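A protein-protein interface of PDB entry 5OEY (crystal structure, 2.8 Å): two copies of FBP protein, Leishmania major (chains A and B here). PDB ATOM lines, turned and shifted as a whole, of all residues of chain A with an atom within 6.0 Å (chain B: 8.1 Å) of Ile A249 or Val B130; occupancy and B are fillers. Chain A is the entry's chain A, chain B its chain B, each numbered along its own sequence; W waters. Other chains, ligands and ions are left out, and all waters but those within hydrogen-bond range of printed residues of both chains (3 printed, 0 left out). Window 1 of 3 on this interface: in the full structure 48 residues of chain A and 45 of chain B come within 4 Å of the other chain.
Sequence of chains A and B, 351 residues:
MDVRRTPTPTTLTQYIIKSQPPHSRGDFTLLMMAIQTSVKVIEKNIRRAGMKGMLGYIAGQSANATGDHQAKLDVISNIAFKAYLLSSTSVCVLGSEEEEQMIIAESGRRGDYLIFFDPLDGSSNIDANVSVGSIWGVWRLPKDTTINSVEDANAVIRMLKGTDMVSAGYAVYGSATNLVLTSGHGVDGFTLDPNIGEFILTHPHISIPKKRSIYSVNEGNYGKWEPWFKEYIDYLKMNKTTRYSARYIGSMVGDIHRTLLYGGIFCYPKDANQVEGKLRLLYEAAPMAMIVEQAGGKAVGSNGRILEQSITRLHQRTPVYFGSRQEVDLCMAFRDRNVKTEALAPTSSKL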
ATOM      1  N   ASN A 125     -16.591 -23.763  13.709  1.00  0.00           N
ATOM      2  CA  ASN A 125     -15.192 -24.107  13.565  1.00  0.00           C
ATOM      3  C   ASN A 125     -14.804 -24.311  12.118  1.00  0.00           C
ATOM      4  O   ASN A 125     -13.619 -24.369  11.811  1.00  0.00           O
ATOM      5  CB  ASN A 125     -14.925 -25.433  14.267  1.00  0.00           C
ATOM      6  CG  ASN A 125     -14.353 -25.274  15.640  1.00  0.00           C
ATOM      7  OD1 ASN A 125     -14.049 -24.185  16.094  1.00  0.00           O
ATOM      8  ND2 ASN A 125     -14.320 -26.362  16.352  1.00  0.00           N
ATOM      9  N   VAL A 130     -11.046 -26.195  11.820  1.00  0.00           N
ATOM     10  CA  VAL A 130     -10.910 -26.837  13.113  1.00  0.00           C
ATOM     11  C   VAL A 130     -11.903 -27.996  13.096  1.00  0.00           C
ATOM     12  O   VAL A 130     -12.946 -27.917  12.444  1.00  0.00           O
ATOM     13  CB  VAL A 130     -11.221 -25.836  14.248  1.00  0.00           C
ATOM     14  CG1 VAL A 130     -11.164 -26.498  15.626  1.00  0.00           C
ATOM     15  CG2 VAL A 130     -10.238 -24.661  14.162  1.00  0.00           C
ATOM     16  N   SER A 131     -11.597 -29.064  13.832  1.00  0.00           N
ATOM     17  CA  SER A 131     -12.401 -30.271  13.734  1.00  0.00           C
ATOM     18  C   SER A 131     -13.870 -30.059  14.125  1.00  0.00           C
ATOM     19  O   SER A 131     -14.225 -29.148  14.873  1.00  0.00           O
ATOM     20  CB  SER A 131     -11.780 -31.468  14.496  1.00  0.00           C
ATOM     21  OG  SER A 131     -11.507 -31.166  15.847  1.00  0.00           O
ATOM     22  N   SER A 175      -8.305 -34.656   9.840  1.00  0.00           N
ATOM     23  CA  SER A 175      -7.330 -35.083   8.845  1.00  0.00           C
ATOM     24  C   SER A 175      -7.655 -36.503   8.432  1.00  0.00           C
ATOM     25  O   SER A 175      -7.400 -36.889   7.284  1.00  0.00           O
ATOM     26  CB  SER A 175      -5.860 -35.063   9.379  1.00  0.00           C
ATOM     27  OG  SER A 175      -5.563 -34.201  10.526  1.00  0.00           O
ATOM     28  N   SER A 216      -9.865 -29.729  29.897  1.00  0.00           N
ATOM     29  CA  SER A 216     -10.470 -29.101  28.727  1.00  0.00           C
ATOM     30  C   SER A 216     -11.734 -28.319  29.104  1.00  0.00           C
ATOM     31  O   SER A 216     -12.756 -28.888  29.511  1.00  0.00           O
ATOM     32  CB  SER A 216     -10.782 -30.167  27.670  1.00  0.00           C
ATOM     33  OG  SER A 216     -11.051 -29.603  26.394  1.00  0.00           O
ATOM     34  N   ARG A 247      -6.034 -28.121  27.049  1.00  0.00           N
ATOM     35  CA  ARG A 247      -6.404 -28.247  25.643  1.00  0.00           C
ATOM     36  C   ARG A 247      -7.903 -27.988  25.482  1.00  0.00           C
ATOM     37  O   ARG A 247      -8.709 -28.649  26.134  1.00  0.00           O
ATOM     38  CB  ARG A 247      -6.116 -29.667  25.095  1.00  0.00           C
ATOM     39  CG  ARG A 247      -4.650 -30.032  24.978  1.00  0.00           C
ATOM     40  CD  ARG A 247      -3.960 -29.230  23.892  1.00  0.00           C
ATOM     41  NE  ARG A 247      -2.577 -29.668  23.753  1.00  0.00           N
ATOM     42  CZ  ARG A 247      -1.557 -29.282  24.533  1.00  0.00           C
ATOM     43  NH1 ARG A 247      -1.706 -28.396  25.528  1.00  0.00           N
ATOM     44  NH2 ARG A 247      -0.350 -29.763  24.290  1.00  0.00           N
ATOM     45  N   TYR A 248      -8.254 -27.052  24.598  1.00  0.00           N
ATOM     46  CA  TYR A 248      -9.639 -26.798  24.246  1.00  0.00           C
ATOM     47  C   TYR A 248      -9.727 -26.404  22.755  1.00  0.00           C
ATOM     48  O   TYR A 248      -9.483 -25.253  22.366  1.00  0.00           O
ATOM     49  CB  TYR A 248     -10.215 -25.719  25.154  1.00  0.00           C
ATOM     50  CG  TYR A 248     -11.721 -25.580  25.100  1.00  0.00           C
ATOM     51  CD1 TYR A 248     -12.535 -26.545  25.649  1.00  0.00           C
ATOM     52  CD2 TYR A 248     -12.328 -24.446  24.555  1.00  0.00           C
ATOM     53  CE1 TYR A 248     -13.916 -26.407  25.641  1.00  0.00           C
ATOM     54  CE2 TYR A 248     -13.709 -24.307  24.521  1.00  0.00           C
ATOM     55  CZ  TYR A 248     -14.494 -25.295  25.079  1.00  0.00           C
ATOM     56  OH  TYR A 248     -15.854 -25.183  25.091  1.00  0.00           O
ATOM     57  N   ILE A 249     -10.035 -27.407  21.939  1.00  0.00           N
ATOM     58  CA  ILE A 249     -10.281 -27.244  20.511  1.00  0.00           C
ATOM     59  C   ILE A 249     -11.537 -26.401  20.277  1.00  0.00           C
ATOM     60  O   ILE A 249     -11.582 -25.600  19.347  1.00  0.00           O
ATOM     61  CB  ILE A 249     -10.474 -28.612  19.818  1.00  0.00           C
ATOM     62  CG1 ILE A 249      -9.216 -29.461  19.905  1.00  0.00           C
ATOM     63  CG2 ILE A 249     -10.824 -28.450  18.341  1.00  0.00           C
ATOM     64  CD1 ILE A 249      -9.514 -30.936  19.841  1.00  0.00           C
ATOM     65  N   GLY A 250     -12.519 -26.551  21.151  1.00  0.00           N
ATOM     66  CA  GLY A 250     -13.793 -25.863  21.014  1.00  0.00           C
ATOM     67  C   GLY A 250     -14.788 -26.644  20.183  1.00  0.00           C
ATOM     68  O   GLY A 250     -15.759 -26.092  19.710  1.00  0.00           O
ATOM     69  N   SER A 251     -14.510 -27.914  19.943  1.00  0.00           N
ATOM     70  CA  SER A 251     -15.436 -28.798  19.270  1.00  0.00           C
ATOM     71  C   SER A 251     -15.651 -29.900  20.244  1.00  0.00           C
ATOM     72  O   SER A 251     -14.690 -30.535  20.650  1.00  0.00           O
ATOM     73  CB  SER A 251     -14.818 -29.370  17.999  1.00  0.00           C
ATOM     74  OG  SER A 251     -15.812 -30.002  17.238  1.00  0.00           O
ATOM     75  N   GLY A 254     -14.313 -33.194  18.971  1.00  0.00           N
ATOM     76  CA  GLY A 254     -12.845 -33.197  18.931  1.00  0.00           C
ATOM     77  C   GLY A 254     -12.208 -33.373  20.291  1.00  0.00           C
ATOM     78  O   GLY A 254     -11.306 -34.198  20.462  1.00  0.00           O
ATOM     79  N   ASP A 255     -12.704 -32.592  21.251  1.00  0.00           N
ATOM     80  CA  ASP A 255     -12.200 -32.569  22.633  1.00  0.00           C
ATOM     81  C   ASP A 255     -12.497 -33.875  23.372  1.00  0.00           C
ATOM     82  O   ASP A 255     -11.629 -34.374  24.084  1.00  0.00           O
ATOM     83  CB  ASP A 255     -12.776 -31.360  23.415  1.00  0.00           C
ATOM     84  CG  ASP A 255     -12.123 -30.015  23.023  1.00  0.00           C
ATOM     85  OD1 ASP A 255     -10.863 -29.955  22.949  1.00  0.00           O
ATOM     86  OD2 ASP A 255     -12.858 -29.014  22.805  1.00  0.00           O
ATOM     87  N   ARG A 258     -10.248 -36.672  21.946  1.00  0.00           N
ATOM     88  CA  ARG A 258      -8.921 -36.570  22.572  1.00  0.00           C
ATOM     89  C   ARG A 258      -8.998 -37.052  24.017  1.00  0.00           C
ATOM     90  O   ARG A 258      -8.108 -37.763  24.460  1.00  0.00           O
ATOM     91  CB  ARG A 258      -8.374 -35.153  22.527  1.00  0.00           C
ATOM     92  CG  ARG A 258      -6.921 -35.028  22.999  1.00  0.00           C
ATOM     93  CD  ARG A 258      -6.556 -33.639  23.537  1.00  0.00           C
ATOM     94  NE  ARG A 258      -7.569 -33.153  24.486  1.00  0.00           N
ATOM     95  CZ  ARG A 258      -8.466 -32.197  24.248  1.00  0.00           C
ATOM     96  NH1 ARG A 258      -8.505 -31.530  23.092  1.00  0.00           N
ATOM     97  NH2 ARG A 258      -9.356 -31.902  25.182  1.00  0.00           N
ATOM     98  N   ILE B  46      -1.470 -39.151   6.297  1.00  0.00           N
ATOM     99  CA  ILE B  46      -2.218 -38.856   7.508  1.00  0.00           C
ATOM    100  C   ILE B  46      -3.639 -39.434   7.449  1.00  0.00           C
ATOM    101  O   ILE B  46      -4.106 -40.023   8.398  1.00  0.00           O
ATOM    102  CB  ILE B  46      -2.261 -37.340   7.798  1.00  0.00           C
ATOM    103  CG1 ILE B  46      -0.855 -36.827   8.087  1.00  0.00           C
ATOM    104  CG2 ILE B  46      -3.138 -37.040   9.016  1.00  0.00           C
ATOM    105  CD1 ILE B  46      -0.740 -35.337   7.889  1.00  0.00           C
ATOM    106  N   ASP B 121       3.985 -30.423  11.961  1.00  0.00           N
ATOM    107  CA  ASP B 121       3.789 -29.664  13.178  1.00  0.00           C
ATOM    108  C   ASP B 121       2.597 -30.218  13.926  1.00  0.00           C
ATOM    109  O   ASP B 121       1.540 -30.384  13.358  1.00  0.00           O
ATOM    110  CB  ASP B 121       3.555 -28.184  12.863  1.00  0.00           C
ATOM    111  CG  ASP B 121       3.133 -27.383  14.090  1.00  0.00           C
ATOM    112  OD1 ASP B 121       3.994 -27.134  14.984  1.00  0.00           O
ATOM    113  OD2 ASP B 121       1.944 -26.991  14.150  1.00  0.00           O
ATOM    114  N   GLY B 122       2.801 -30.487  15.206  1.00  0.00           N
ATOM    115  CA  GLY B 122       1.787 -31.007  16.070  1.00  0.00           C
ATOM    116  C   GLY B 122       1.731 -32.511  16.044  1.00  0.00           C
ATOM    117  O   GLY B 122       0.728 -33.064  16.432  1.00  0.00           O
ATOM    118  N   SER B 123       2.840 -33.185  15.740  1.00  0.00           N
ATOM    119  CA  SER B 123       2.831 -34.654  15.542  1.00  0.00           C
ATOM    120  C   SER B 123       2.294 -35.497  16.697  1.00  0.00           C
ATOM    121  O   SER B 123       1.847 -36.606  16.475  1.00  0.00           O
ATOM    122  CB  SER B 123       4.220 -35.191  15.146  1.00  0.00           C
ATOM    123  OG  SER B 123       5.221 -34.178  15.220  1.00  0.00           O
ATOM    124  N   SER B 124       2.326 -34.977  17.919  1.00  0.00           N
ATOM    125  CA  SER B 124       1.664 -35.613  19.064  1.00  0.00           C
ATOM    126  C   SER B 124       0.123 -35.338  19.163  1.00  0.00           C
ATOM    127  O   SER B 124      -0.516 -35.492  20.236  1.00  0.00           O
ATOM    128  CB  SER B 124       2.340 -35.104  20.327  1.00  0.00           C
ATOM    129  OG  SER B 124       2.121 -33.707  20.430  1.00  0.00           O
ATOM    130  N   ASN B 125      -0.461 -34.887  18.066  1.00  0.00           N
ATOM    131  CA  ASN B 125      -1.885 -34.668  17.949  1.00  0.00           C
ATOM    132  C   ASN B 125      -2.546 -35.732  17.087  1.00  0.00           C
ATOM    133  O   ASN B 125      -3.758 -35.836  17.073  1.00  0.00           O
ATOM    134  CB  ASN B 125      -2.126 -33.301  17.285  1.00  0.00           C
ATOM    135  CG  ASN B 125      -2.266 -32.166  18.283  1.00  0.00           C
ATOM    136  OD1 ASN B 125      -2.551 -32.400  19.450  1.00  0.00           O
ATOM    137  ND2 ASN B 125      -2.347 -30.951  17.768  1.00  0.00           N
ATOM    138  N   ILE B 126      -1.757 -36.501  16.351  1.00  0.00           N
ATOM    139  CA  ILE B 126      -2.277 -37.245  15.225  1.00  0.00           C
ATOM    140  C   ILE B 126      -3.108 -38.411  15.747  1.00  0.00           C
ATOM    141  O   ILE B 126      -4.202 -38.676  15.247  1.00  0.00           O
ATOM    142  CB  ILE B 126      -1.172 -37.806  14.318  1.00  0.00           C
ATOM    143  CG1 ILE B 126      -0.130 -36.701  13.925  1.00  0.00           C
ATOM    144  CG2 ILE B 126      -1.816 -38.439  13.087  1.00  0.00           C
ATOM    145  CD1 ILE B 126      -0.176 -36.211  12.478  1.00  0.00           C
ATOM    146  N   ASP B 127      -2.567 -39.114  16.731  1.00  0.00           N
ATOM    147  CA  ASP B 127      -3.273 -40.227  17.358  1.00  0.00           C
ATOM    148  C   ASP B 127      -4.682 -39.855  17.867  1.00  0.00           C
ATOM    149  O   ASP B 127      -5.557 -40.728  17.926  1.00  0.00           O
ATOM    150  CB  ASP B 127      -2.401 -40.962  18.412  1.00  0.00           C
ATOM    151  CG  ASP B 127      -1.769 -40.020  19.419  1.00  0.00           C
ATOM    152  OD1 ASP B 127      -1.988 -38.779  19.306  1.00  0.00           O
ATOM    153  OD2 ASP B 127      -1.054 -40.525  20.337  1.00  0.00           O
ATOM    154  N   ALA B 128      -4.914 -38.575  18.178  1.00  0.00           N
ATOM    155  CA  ALA B 128      -6.254 -38.089  18.576  1.00  0.00           C
ATOM    156  C   ALA B 128      -7.031 -37.318  17.504  1.00  0.00           C
ATOM    157  O   ALA B 128      -8.046 -36.682  17.803  1.00  0.00           O
ATOM    158  CB  ALA B 128      -6.132 -37.246  19.831  1.00  0.00           C
ATOM    159  N   ASN B 129      -6.570 -37.403  16.263  1.00  0.00           N
ATOM    160  CA  ASN B 129      -7.177 -36.726  15.117  1.00  0.00           C
ATOM    161  C   ASN B 129      -7.379 -35.228  15.301  1.00  0.00           C
ATOM    162  O   ASN B 129      -8.367 -34.656  14.815  1.00  0.00           O
ATOM    163  CB  ASN B 129      -8.509 -37.370  14.755  1.00  0.00           C
ATOM    164  CG  ASN B 129      -8.911 -37.133  13.305  1.00  0.00           C
ATOM    165  OD1 ASN B 129      -8.114 -36.696  12.470  1.00  0.00           O
ATOM    166  ND2 ASN B 129     -10.152 -37.447  12.997  1.00  0.00           N
ATOM    167  N   VAL B 130      -6.435 -34.604  15.989  1.00  0.00           N
ATOM    168  CA  VAL B 130      -6.411 -33.168  16.167  1.00  0.00           C
ATOM    169  C   VAL B 130      -5.508 -32.604  15.061  1.00  0.00           C
ATOM    170  O   VAL B 130      -4.626 -33.301  14.571  1.00  0.00           O
ATOM    171  CB  VAL B 130      -5.871 -32.803  17.556  1.00  0.00           C
ATOM    172  CG1 VAL B 130      -5.792 -31.293  17.731  1.00  0.00           C
ATOM    173  CG2 VAL B 130      -6.721 -33.424  18.650  1.00  0.00           C
ATOM    174  N   SER B 131      -5.790 -31.387  14.602  1.00  0.00           N
ATOM    175  CA  SER B 131      -5.156 -30.899  13.385  1.00  0.00           C
ATOM    176  C   SER B 131      -3.651 -30.794  13.533  1.00  0.00           C
ATOM    177  O   SER B 131      -3.125 -30.708  14.636  1.00  0.00           O
ATOM    178  CB  SER B 131      -5.771 -29.575  12.874  1.00  0.00           C
ATOM    179  OG  SER B 131      -5.862 -28.605  13.888  1.00  0.00           O
ATOM    180  N   VAL B 132      -2.979 -30.902  12.392  1.00  0.00           N
ATOM    181  CA  VAL B 132      -1.543 -30.821  12.300  1.00  0.00           C
ATOM    182  C   VAL B 132      -1.248 -30.044  11.030  1.00  0.00           C
ATOM    183  O   VAL B 132      -2.169 -29.690  10.290  1.00  0.00           O
ATOM    184  CB  VAL B 132      -0.895 -32.217  12.257  1.00  0.00           C
ATOM    185  CG1 VAL B 132      -1.090 -32.913  13.575  1.00  0.00           C
ATOM    186  CG2 VAL B 132      -1.462 -33.073  11.137  1.00  0.00           C
ATOM    187  N   GLY B 133       0.018 -29.739  10.788  1.00  0.00           N
ATOM    188  CA  GLY B 133       0.384 -28.892   9.674  1.00  0.00           C
ATOM    189  C   GLY B 133       1.817 -29.064   9.229  1.00  0.00           C
ATOM    190  O   GLY B 133       2.551 -29.855   9.791  1.00  0.00           O
ATOM    191  N   VAL B 172      -2.454 -26.801   6.525  1.00  0.00           N
ATOM    192  CA  VAL B 172      -3.260 -27.392   7.589  1.00  0.00           C
ATOM    193  C   VAL B 172      -3.899 -28.668   7.116  1.00  0.00           C
ATOM    194  O   VAL B 172      -4.637 -28.662   6.128  1.00  0.00           O
ATOM    195  CB  VAL B 172      -4.433 -26.501   8.033  1.00  0.00           C
ATOM    196  CG1 VAL B 172      -4.943 -26.946   9.403  1.00  0.00           C
ATOM    197  CG2 VAL B 172      -4.011 -25.049   8.097  1.00  0.00           C
ATOM    198  N   TYR B 173      -3.673 -29.743   7.881  1.00  0.00           N
ATOM    199  CA  TYR B 173      -4.268 -31.055   7.586  1.00  0.00           C
ATOM    200  C   TYR B 173      -5.417 -31.252   8.563  1.00  0.00           C
ATOM    201  O   TYR B 173      -5.219 -31.545   9.754  1.00  0.00           O
ATOM    202  CB  TYR B 173      -3.249 -32.169   7.700  1.00  0.00           C
ATOM    203  CG  TYR B 173      -1.991 -31.922   6.906  1.00  0.00           C
ATOM    204  CD1 TYR B 173      -1.941 -32.166   5.540  1.00  0.00           C
ATOM    205  CD2 TYR B 173      -0.832 -31.464   7.540  1.00  0.00           C
ATOM    206  CE1 TYR B 173      -0.782 -31.943   4.808  1.00  0.00           C
ATOM    207  CE2 TYR B 173       0.338 -31.252   6.831  1.00  0.00           C
ATOM    208  CZ  TYR B 173       0.365 -31.488   5.458  1.00  0.00           C
ATOM    209  OH  TYR B 173       1.519 -31.284   4.751  1.00  0.00           O
ATOM    210  N   GLY B 174      -6.616 -31.001   8.052  1.00  0.00           N
ATOM    211  CA  GLY B 174      -7.835 -31.131   8.824  1.00  0.00           C
ATOM    212  C   GLY B 174      -8.891 -31.767   7.940  1.00  0.00           C
ATOM    213  O   GLY B 174      -8.572 -32.533   7.009  1.00  0.00           O
ATOM    214  N   ALA B 246     -11.768 -18.456  24.843  1.00  0.00           N
ATOM    215  CA  ALA B 246     -10.491 -19.164  24.862  1.00  0.00           C
ATOM    216  C   ALA B 246     -10.548 -20.349  23.929  1.00  0.00           C
ATOM    217  O   ALA B 246     -11.509 -21.108  23.949  1.00  0.00           O
ATOM    218  CB  ALA B 246     -10.146 -19.629  26.265  1.00  0.00           C
ATOM    219  N   ARG B 247      -9.508 -20.490  23.106  1.00  0.00           N
ATOM    220  CA  ARG B 247      -9.342 -21.629  22.204  1.00  0.00           C
ATOM    221  C   ARG B 247      -7.888 -22.004  22.126  1.00  0.00           C
ATOM    222  O   ARG B 247      -7.040 -21.163  21.824  1.00  0.00           O
ATOM    223  CB  ARG B 247      -9.810 -21.296  20.786  1.00  0.00           C
ATOM    224  CG  ARG B 247     -11.302 -21.084  20.616  1.00  0.00           C
ATOM    225  CD  ARG B 247     -12.065 -22.375  20.810  1.00  0.00           C
ATOM    226  NE  ARG B 247     -13.486 -22.174  20.548  1.00  0.00           N
ATOM    227  CZ  ARG B 247     -14.359 -21.643  21.401  1.00  0.00           C
ATOM    228  NH1 ARG B 247     -14.017 -21.303  22.651  1.00  0.00           N
ATOM    229  NH2 ARG B 247     -15.602 -21.475  21.005  1.00  0.00           N
ATOM    230  N   TYR B 248      -7.593 -23.271  22.413  1.00  0.00           N
ATOM    231  CA  TYR B 248      -6.227 -23.818  22.268  1.00  0.00           C
ATOM    232  C   TYR B 248      -6.286 -25.278  21.781  1.00  0.00           C
ATOM    233  O   TYR B 248      -6.528 -26.208  22.559  1.00  0.00           O
ATOM    234  CB  TYR B 248      -5.465 -23.678  23.584  1.00  0.00           C
ATOM    235  CG  TYR B 248      -3.974 -23.893  23.483  1.00  0.00           C
ATOM    236  CD1 TYR B 248      -3.163 -22.984  22.819  1.00  0.00           C
ATOM    237  CD2 TYR B 248      -3.362 -25.020  24.049  1.00  0.00           C
ATOM    238  CE1 TYR B 248      -1.800 -23.190  22.715  1.00  0.00           C
ATOM    239  CE2 TYR B 248      -1.994 -25.237  23.944  1.00  0.00           C
ATOM    240  CZ  TYR B 248      -1.216 -24.314  23.289  1.00  0.00           C
ATOM    241  OH  TYR B 248       0.144 -24.480  23.220  1.00  0.00           O
ATOM    242  N   ILE B 249      -6.156 -25.435  20.467  1.00  0.00           N
ATOM    243  CA  ILE B 249      -6.113 -26.740  19.823  1.00  0.00           C
ATOM    244  C   ILE B 249      -4.855 -27.481  20.233  1.00  0.00           C
ATOM    245  O   ILE B 249      -4.866 -28.694  20.398  1.00  0.00           O
ATOM    246  CB  ILE B 249      -6.123 -26.605  18.286  1.00  0.00           C
ATOM    247  CG1 ILE B 249      -7.449 -25.980  17.787  1.00  0.00           C
ATOM    248  CG2 ILE B 249      -5.946 -27.956  17.588  1.00  0.00           C
ATOM    249  CD1 ILE B 249      -7.276 -25.242  16.469  1.00  0.00           C
ATOM    250  N   GLY B 250      -3.773 -26.737  20.413  1.00  0.00           N
ATOM    251  CA  GLY B 250      -2.475 -27.330  20.728  1.00  0.00           C
ATOM    252  C   GLY B 250      -1.694 -27.700  19.484  1.00  0.00           C
ATOM    253  O   GLY B 250      -0.724 -28.417  19.560  1.00  0.00           O
ATOM    254  N   SER B 251      -2.105 -27.199  18.336  1.00  0.00           N
ATOM    255  CA  SER B 251      -1.338 -27.321  17.109  1.00  0.00           C
ATOM    256  C   SER B 251      -1.087 -25.909  16.686  1.00  0.00           C
ATOM    257  O   SER B 251      -2.015 -25.164  16.485  1.00  0.00           O
ATOM    258  CB  SER B 251      -2.149 -28.010  16.006  1.00  0.00           C
ATOM    259  OG  SER B 251      -1.308 -28.386  14.930  1.00  0.00           O
ATOM    260  N   GLY B 254      -2.855 -25.092  13.415  1.00  0.00           N
ATOM    261  CA  GLY B 254      -4.305 -25.018  13.602  1.00  0.00           C
ATOM    262  C   GLY B 254      -4.753 -23.740  14.291  1.00  0.00           C
ATOM    263  O   GLY B 254      -5.674 -23.070  13.814  1.00  0.00           O
ATOM    264  N   ASP B 255      -4.071 -23.401  15.393  1.00  0.00           N
ATOM    265  CA  ASP B 255      -4.366 -22.217  16.213  1.00  0.00           C
ATOM    266  C   ASP B 255      -4.070 -20.908  15.481  1.00  0.00           C
ATOM    267  O   ASP B 255      -4.868 -19.970  15.551  1.00  0.00           O
ATOM    268  CB  ASP B 255      -3.598 -22.259  17.554  1.00  0.00           C
ATOM    269  CG  ASP B 255      -4.185 -23.263  18.550  1.00  0.00           C
ATOM    270  OD1 ASP B 255      -5.432 -23.270  18.742  1.00  0.00           O
ATOM    271  OD2 ASP B 255      -3.410 -24.047  19.174  1.00  0.00           O
ATOM    272  N   ARG B 258      -6.693 -20.376  12.675  1.00  0.00           N
ATOM    273  CA  ARG B 258      -7.913 -19.811  13.288  1.00  0.00           C
ATOM    274  C   ARG B 258      -7.681 -18.360  13.630  1.00  0.00           C
ATOM    275  O   ARG B 258      -8.551 -17.544  13.394  1.00  0.00           O
ATOM    276  CB  ARG B 258      -8.351 -20.584  14.532  1.00  0.00           C
ATOM    277  CG  ARG B 258      -9.707 -20.159  15.092  1.00  0.00           C
ATOM    278  CD  ARG B 258      -9.894 -20.451  16.578  1.00  0.00           C
ATOM    279  NE  ARG B 258      -8.739 -20.010  17.360  1.00  0.00           N
ATOM    280  CZ  ARG B 258      -7.813 -20.802  17.913  1.00  0.00           C
ATOM    281  NH1 ARG B 258      -7.874 -22.139  17.838  1.00  0.00           N
ATOM    282  NH2 ARG B 258      -6.786 -20.240  18.551  1.00  0.00           N
HETATM  283  O   HOH W   1      -7.652 -33.218  12.292  1.00  0.00           O
HETATM  284  O   HOH W   2      -3.612 -32.113  22.154  1.00  0.00           O
HETATM  285  O   HOH W   3      -6.278 -31.220  21.421  1.00  0.00           O
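The side-chain hydroxyl (OG) of Ser A175 is in hydrogen-bond range of the backbone carbonyl oxygen (O) of Tyr B173 (2.8 Å). N of Ser A175 sits at hydrogen-bond distance from OD1 of Asn B129 (3.3 Å). O of Tyr A248 is in hydrogen-bond range of N of Tyr B248 (2.7 Å).
N of Tyr B173 sits at hydrogen-bond distance from O of Val B132 (2.8 Å). The backbone carbonyl oxygen (O) of Asn B125 sits at hydrogen-bond distance from the backbone NH (N) of Val B130, at 3.1 Å. The side-chain carboxylate of Asp A255 is in salt-bridge range of the guanidinium group of Arg A258 (2.8 Å). The side-chain hydroxyl of Ser A216 sits at hydrogen-bond distance from the backbone carbonyl oxygen of Arg A247, at 2.5 Å. The backbone NH (N) of Gly B250 is in hydrogen-bond range of the side-chain carboxylate (OD2) of Asp B255 (3.0 Å). The backbone NH (N) of Ile B249 is in hydrogen-bond range of the side-chain carboxylate (OD1) of Asp B255.
Among the printed residues, pairs that only touch across the chains: Ser A175 with Gly B174, Ser A175 with Ile B46, Tyr A248 with Ala B246, Arg A247 with Tyr B248, Tyr A248 with Arg B247, Ile A249 with Arg B247, Arg A247 with Ile B249, Gly A250 with Arg B247, Ile A249 with Tyr B248, Val A130 with Ile B249, Arg A247 with Gly B250, Tyr A248 with Ile B249, Ile A249 with Val B130 and Arg A258 with Ala B128.
Asn A125 touches none of the printed residues of chain B. Of the printed residues of chain B, Val A130 touches Ile B249 (3.8 Å). Printed residues of chain B within 4 Å of Tyr A248: Ala B246 (3.5 Å), Arg B247 (3.6 Å), Tyr B248 (2.7 Å) and Ile B249 (3.8 Å). Printed residues of chain B within 4 Å of Ile A249: Val B130, Arg B247 and Tyr B248. Of the printed residues of chain B, Gly A250 touches Arg B247 (3.7 Å). Of the printed residues of chain A, Ile B46 touches Ser A175 (3.4 Å). Of chain A, only Ile A249 (3.9 Å) comes within 4 Å of Val B130. Of the printed residues of chain A, Gly B250 touches Arg A247. Gly B254 touches none of the printed residues of chain A. The nearest residue of chain B that does not touch Ile A249 is Ile B249 (4.1 Å). The nearest residue of chain A that does not touch Val B130 is Ser A175 (4.2 Å). The nearest printed residue of chain A that does not touch Arg B247 is Asn A125 (4.9 Å).
Of the 13 printed residues of chain A, 7 touch a printed residue of chain B. Hydrophobic or aromatic side chains of chain A within 4 Å of the printed part of chain B: Val A130, Tyr A248 and Ile A249. Along chain B the printed residues that touch a printed residue of chain A span positions 46 to 250. Among the printed residues, 17 pairs touch across the chains.
Arg A247 touches Tyr B248, and with the chains exchanged Tyr A248 touches Arg B247. Arg A247 touches Ile B249, and with the chains exchanged Ile A249 touches Arg B247. Tyr A248 touches its own counterpart, Tyr B248. Tyr A248 touches Ile B249, and with the chains exchanged Ile A249 touches Tyr B248. Positions printed for both chains: 125, 130, 131, 247, 248, 249, 250, 251, 254, 255 and 258.
Water W3 bridges NH1 of Arg A258 (2.8 Å) and O of Ile B249 (3.1 Å). Water W1 lies within hydrogen-bond range of the side-chain hydroxyl (OG) of Ser A175 (2.9 Å), the backbone carbonyl oxygen (O) of Asn B129 (3.0 Å) and the backbone NH (N) of Ser B131 (3.5 Å). Water W2 lies within hydrogen-bond range of the side-chain amide oxygen (OD1) of Asn B125 and the guanidinium group (NE) of Arg A247.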
